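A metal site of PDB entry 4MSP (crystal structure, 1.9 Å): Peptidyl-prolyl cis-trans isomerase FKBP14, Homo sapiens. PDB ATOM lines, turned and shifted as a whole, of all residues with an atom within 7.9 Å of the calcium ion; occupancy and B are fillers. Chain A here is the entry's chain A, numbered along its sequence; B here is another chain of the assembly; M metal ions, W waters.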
ATOM      1  N   PHE A 133      19.426  26.731   9.424  1.00  0.00           N
ATOM      2  CA  PHE A 133      20.326  26.524   8.295  1.00  0.00           C
ATOM      3  C   PHE A 133      20.756  25.060   8.199  1.00  0.00           C
ATOM      4  O   PHE A 133      20.696  24.452   7.128  1.00  0.00           O
ATOM      5  CB  PHE A 133      21.553  27.433   8.420  1.00  0.00           C
ATOM      6  CG  PHE A 133      22.505  27.330   7.249  1.00  0.00           C
ATOM      7  CD1 PHE A 133      22.336  28.121   6.128  1.00  0.00           C
ATOM      8  CD2 PHE A 133      23.564  26.442   7.276  1.00  0.00           C
ATOM      9  CE1 PHE A 133      23.198  28.034   5.061  1.00  0.00           C
ATOM     10  CE2 PHE A 133      24.436  26.348   6.217  1.00  0.00           C
ATOM     11  CZ  PHE A 133      24.250  27.153   5.103  1.00  0.00           C
ATOM     12  N   GLN A 134      21.181  24.504   9.332  1.00  0.00           N
ATOM     13  CA  GLN A 134      21.630  23.110   9.352  1.00  0.00           C
ATOM     14  C   GLN A 134      20.501  22.162   8.961  1.00  0.00           C
ATOM     15  O   GLN A 134      20.731  21.191   8.258  1.00  0.00           O
ATOM     16  CB  GLN A 134      22.179  22.755  10.722  1.00  0.00           C
ATOM     17  CG  GLN A 134      23.485  23.478  11.050  1.00  0.00           C
ATOM     18  CD  GLN A 134      24.065  23.052  12.380  1.00  0.00           C
ATOM     19  OE1 GLN A 134      23.341  22.672  13.293  1.00  0.00           O
ATOM     20  NE2 GLN A 134      25.388  23.090  12.484  1.00  0.00           N
ATOM     21  N   MET A 136      18.093  22.715   6.945  1.00  0.00           N
ATOM     22  CA  MET A 136      17.882  22.837   5.498  1.00  0.00           C
ATOM     23  C   MET A 136      19.041  22.281   4.700  1.00  0.00           C
ATOM     24  O   MET A 136      18.860  21.737   3.613  1.00  0.00           O
ATOM     25  CB  MET A 136      17.639  24.297   5.105  1.00  0.00           C
ATOM     26  CG  MET A 136      16.307  24.849   5.630  1.00  0.00           C
ATOM     27  SD  MET A 136      16.133  26.615   5.290  1.00  0.00           S
ATOM     28  CE  MET A 136      15.642  26.551   3.569  1.00  0.00           C
ATOM     29  N   ASP A 137      20.248  22.422   5.249  1.00  0.00           N
ATOM     30  CA  ASP A 137      21.457  21.986   4.556  1.00  0.00           C
ATOM     31  C   ASP A 137      21.592  20.471   4.622  1.00  0.00           C
ATOM     32  O   ASP A 137      22.401  19.945   5.399  1.00  0.00           O
ATOM     33  CB  ASP A 137      22.688  22.661   5.179  1.00  0.00           C
ATOM     34  CG  ASP A 137      23.961  22.272   4.495  1.00  0.00           C
ATOM     35  OD1 ASP A 137      23.888  21.817   3.337  1.00  0.00           O
ATOM     36  OD2 ASP A 137      25.052  22.421   5.102  1.00  0.00           O
ATOM     37  N   LEU A 138      20.799  19.765   3.802  1.00  0.00           N
ATOM     38  CA  LEU A 138      20.710  18.312   3.872  1.00  0.00           C
ATOM     39  C   LEU A 138      22.044  17.587   3.676  1.00  0.00           C
ATOM     40  O   LEU A 138      22.279  16.552   4.292  1.00  0.00           O
ATOM     41  CB  LEU A 138      19.681  17.776   2.863  1.00  0.00           C
ATOM     42  CG  LEU A 138      18.222  18.250   3.051  1.00  0.00           C
ATOM     43  CD1 LEU A 138      17.316  17.705   1.952  1.00  0.00           C
ATOM     44  CD2 LEU A 138      17.680  17.875   4.412  1.00  0.00           C
ATOM     45  N   ASN A 139      22.926  18.120   2.827  1.00  0.00           N
ATOM     46  CA  ASN A 139      24.177  17.430   2.548  1.00  0.00           C
ATOM     47  C   ASN A 139      25.400  17.982   3.282  1.00  0.00           C
ATOM     48  O   ASN A 139      26.546  17.653   2.938  1.00  0.00           O
ATOM     49  CB  ASN A 139      24.442  17.365   1.034  1.00  0.00           C
ATOM     50  CG  ASN A 139      24.866  18.709   0.462  1.00  0.00           C
ATOM     51  OD1 ASN A 139      24.665  19.753   1.077  1.00  0.00           O
ATOM     52  ND2 ASN A 139      25.438  18.670  -0.737  1.00  0.00           N
ATOM     53  N   ASP A 140      25.157  18.817   4.286  1.00  0.00           N
ATOM     54  CA  ASP A 140      26.213  19.350   5.152  1.00  0.00           C
ATOM     55  C   ASP A 140      27.392  20.001   4.408  1.00  0.00           C
ATOM     56  O   ASP A 140      28.540  19.933   4.880  1.00  0.00           O
ATOM     57  CB  ASP A 140      26.754  18.253   6.079  1.00  0.00           C
ATOM     58  CG  ASP A 140      25.645  17.542   6.841  1.00  0.00           C
ATOM     59  OD1 ASP A 140      24.819  18.214   7.483  1.00  0.00           O
ATOM     60  OD2 ASP A 140      25.605  16.294   6.792  1.00  0.00           O
ATOM     61  N   ASP A 141      27.138  20.626   3.260  1.00  0.00           N
ATOM     62  CA  ASP A 141      28.227  21.315   2.565  1.00  0.00           C
ATOM     63  C   ASP A 141      28.250  22.808   2.870  1.00  0.00           C
ATOM     64  O   ASP A 141      28.938  23.576   2.207  1.00  0.00           O
ATOM     65  CB  ASP A 141      28.244  21.041   1.049  1.00  0.00           C
ATOM     66  CG  ASP A 141      27.006  21.563   0.335  1.00  0.00           C
ATOM     67  OD1 ASP A 141      26.136  22.186   0.966  1.00  0.00           O
ATOM     68  OD2 ASP A 141      26.911  21.347  -0.897  1.00  0.00           O
ATOM     69  N   TRP A 142      27.488  23.200   3.892  1.00  0.00           N
ATOM     70  CA  TRP A 142      27.439  24.577   4.387  1.00  0.00           C
ATOM     71  C   TRP A 142      26.918  25.584   3.368  1.00  0.00           C
ATOM     72  O   TRP A 142      27.217  26.777   3.449  1.00  0.00           O
ATOM     73  CB  TRP A 142      28.795  25.021   4.967  1.00  0.00           C
ATOM     74  CG  TRP A 142      29.143  24.309   6.230  1.00  0.00           C
ATOM     75  CD1 TRP A 142      30.127  23.387   6.416  1.00  0.00           C
ATOM     76  CD2 TRP A 142      28.491  24.451   7.505  1.00  0.00           C
ATOM     77  NE1 TRP A 142      30.144  22.954   7.721  1.00  0.00           N
ATOM     78  CE2 TRP A 142      29.136  23.581   8.408  1.00  0.00           C
ATOM     79  CE3 TRP A 142      27.413  25.229   7.962  1.00  0.00           C
ATOM     80  CZ2 TRP A 142      28.750  23.476   9.742  1.00  0.00           C
ATOM     81  CZ3 TRP A 142      27.034  25.113   9.291  1.00  0.00           C
ATOM     82  CH2 TRP A 142      27.699  24.250  10.165  1.00  0.00           C
ATOM     83  N   LYS A 143      26.142  25.089   2.409  1.00  0.00           N
ATOM     84  CA  LYS A 143      25.365  25.964   1.529  1.00  0.00           C
ATOM     85  C   LYS A 143      24.055  25.281   1.163  1.00  0.00           C
ATOM     86  O   LYS A 143      23.936  24.054   1.199  1.00  0.00           O
ATOM     87  CB  LYS A 143      26.166  26.374   0.281  1.00  0.00           C
ATOM     88  CG  LYS A 143      26.497  25.241  -0.664  1.00  0.00           C
ATOM     89  CD  LYS A 143      27.652  25.616  -1.590  1.00  0.00           C
ATOM     90  CE  LYS A 143      28.054  24.441  -2.455  1.00  0.00           C
ATOM     91  NZ  LYS A 143      29.329  24.681  -3.198  1.00  0.00           N
ATOM     92  N   LEU A 144      23.052  26.100   0.835  1.00  0.00           N
ATOM     93  CA  LEU A 144      21.732  25.566   0.522  1.00  0.00           C
ATOM     94  C   LEU A 144      21.523  25.587  -0.979  1.00  0.00           C
ATOM     95  O   LEU A 144      21.565  26.654  -1.592  1.00  0.00           O
ATOM     96  CB  LEU A 144      20.666  26.435   1.181  1.00  0.00           C
ATOM     97  CG  LEU A 144      20.890  26.733   2.663  1.00  0.00           C
ATOM     98  CD1 LEU A 144      19.738  27.545   3.222  1.00  0.00           C
ATOM     99  CD2 LEU A 144      21.056  25.440   3.431  1.00  0.00           C
ATOM    100  N   SER A 145      21.321  24.413  -1.572  1.00  0.00           N
ATOM    101  CA  SER A 145      21.011  24.330  -2.997  1.00  0.00           C
ATOM    102  C   SER A 145      19.547  24.695  -3.214  1.00  0.00           C
ATOM    103  O   SER A 145      18.768  24.746  -2.249  1.00  0.00           O
ATOM    104  CB  SER A 145      21.256  22.923  -3.526  1.00  0.00           C
ATOM    105  OG  SER A 145      20.415  21.993  -2.856  1.00  0.00           O
ATOM    106  N   LYS A 146      19.159  24.938  -4.457  1.00  0.00           N
ATOM    107  CA  LYS A 146      17.767  25.206  -4.758  1.00  0.00           C
ATOM    108  C   LYS A 146      16.914  24.009  -4.375  1.00  0.00           C
ATOM    109  O   LYS A 146      15.788  24.158  -3.911  1.00  0.00           O
ATOM    110  CB  LYS A 146      17.581  25.569  -6.234  1.00  0.00           C
ATOM    111  CG  LYS A 146      18.180  26.914  -6.609  1.00  0.00           C
ATOM    112  CD  LYS A 146      17.960  27.262  -8.080  1.00  0.00           C
ATOM    113  CE  LYS A 146      18.740  28.508  -8.475  1.00  0.00           C
ATOM    114  NZ  LYS A 146      18.521  28.879  -9.893  1.00  0.00           N
ATOM    115  N   GLU A 148      17.480  21.875  -1.943  1.00  0.00           N
ATOM    116  CA  GLU A 148      17.325  21.818  -0.480  1.00  0.00           C
ATOM    117  C   GLU A 148      16.258  22.802  -0.011  1.00  0.00           C
ATOM    118  O   GLU A 148      15.430  22.479   0.861  1.00  0.00           O
ATOM    119  CB  GLU A 148      18.670  22.084   0.209  1.00  0.00           C
ATOM    120  CG  GLU A 148      19.623  20.902   0.102  1.00  0.00           C
ATOM    121  CD  GLU A 148      21.041  21.245   0.509  1.00  0.00           C
ATOM    122  OE1 GLU A 148      21.338  22.456   0.630  1.00  0.00           O
ATOM    123  OE2 GLU A 148      21.860  20.317   0.715  1.00  0.00           O
ATOM    124  N   PHE A 187      23.750  28.768  -4.995  1.00  0.00           N
ATOM    125  CA  PHE A 187      23.622  28.344  -3.611  1.00  0.00           C
ATOM    126  C   PHE A 187      23.468  29.531  -2.676  1.00  0.00           C
ATOM    127  O   PHE A 187      23.791  30.663  -3.023  1.00  0.00           O
ATOM    128  CB  PHE A 187      24.846  27.537  -3.169  1.00  0.00           C
ATOM    129  CG  PHE A 187      25.119  26.337  -4.023  1.00  0.00           C
ATOM    130  CD1 PHE A 187      26.013  26.418  -5.085  1.00  0.00           C
ATOM    131  CD2 PHE A 187      24.498  25.122  -3.755  1.00  0.00           C
ATOM    132  CE1 PHE A 187      26.275  25.314  -5.865  1.00  0.00           C
ATOM    133  CE2 PHE A 187      24.751  24.021  -4.535  1.00  0.00           C
ATOM    134  CZ  PHE A 187      25.638  24.112  -5.592  1.00  0.00           C
ATOM    135  N   ILE A 188      22.975  29.256  -1.479  1.00  0.00           N
ATOM    136  CA  ILE A 188      22.963  30.249  -0.419  1.00  0.00           C
ATOM    137  C   ILE A 188      23.939  29.775   0.652  1.00  0.00           C
ATOM    138  O   ILE A 188      23.611  28.897   1.464  1.00  0.00           O
ATOM    139  CB  ILE A 188      21.563  30.416   0.160  1.00  0.00           C
ATOM    140  CG1 ILE A 188      20.591  30.874  -0.929  1.00  0.00           C
ATOM    141  CG2 ILE A 188      21.570  31.403   1.326  1.00  0.00           C
ATOM    142  CD1 ILE A 188      19.142  30.858  -0.492  1.00  0.00           C
ATOM    143  N   LYS B  30      15.865  16.218   7.303  1.00  0.00           N
ATOM    144  CA  LYS B  30      16.507  16.308   8.623  1.00  0.00           C
ATOM    145  C   LYS B  30      15.486  16.587   9.716  1.00  0.00           C
ATOM    146  O   LYS B  30      14.517  17.328   9.497  1.00  0.00           O
ATOM    147  CB  LYS B  30      17.590  17.394   8.638  1.00  0.00           C
ATOM    148  CG  LYS B  30      18.948  16.981   8.030  1.00  0.00           C
ATOM    149  CD  LYS B  30      19.945  18.130   8.169  1.00  0.00           C
ATOM    150  CE  LYS B  30      21.365  17.722   7.749  1.00  0.00           C
ATOM    151  NZ  LYS B  30      22.369  18.782   8.067  1.00  0.00           N
HETATM  152 CA    CA M   1      23.779  21.858   1.053  1.00  0.00          CA
HETATM  153  O   HOH W   1      24.230  21.824  -1.349  1.00  0.00           O
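The backbone NH (N) of Glu 148 lies within hydrogen-bond range of the side-chain hydroxyl (OG) of Ser 145.
OE2 of Glu 148 sits close to N of Leu 138 (3.3 Å).
The side-chain carboxylate (OD2) of Asp 137 lies within hydrogen-bond range of the backbone NH (N) of Trp 142, at 2.8 Å.
The backbone NH of Asp 140 lies close to the side-chain carboxylate of Asp 137 (3.4 Å).
The backbone carbonyl oxygen of Asp 137 is in hydrogen-bond range of the side-chain amino group of Lys 30 of chain B, at 2.9 Å.
Of the 17 residues printed, 5 come within 4 Å of the calcium ion.
The nearest printed residue that does not touch the calcium ion is Leu 144 (4.3 Å).
The calcium ion is bound by the backbone carbonyl oxygen (O) of Lys 143, the side-chain amide oxygen (OD1) of Asn 139, the side-chain carboxylate (OD1) of Asp 137, the side-chain carboxylate (OD1) of Asp 141, water W1, the side-chain carboxylate (OE2) of Glu 148 and the side-chain carboxylate (OE1) of Glu 148.
The calcium ion has seven donor atoms within binding distance.
Water W1 bridges OD2 of Asp 141 (2.8 Å) and ND2 of Asn 139 (3.4 Å).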
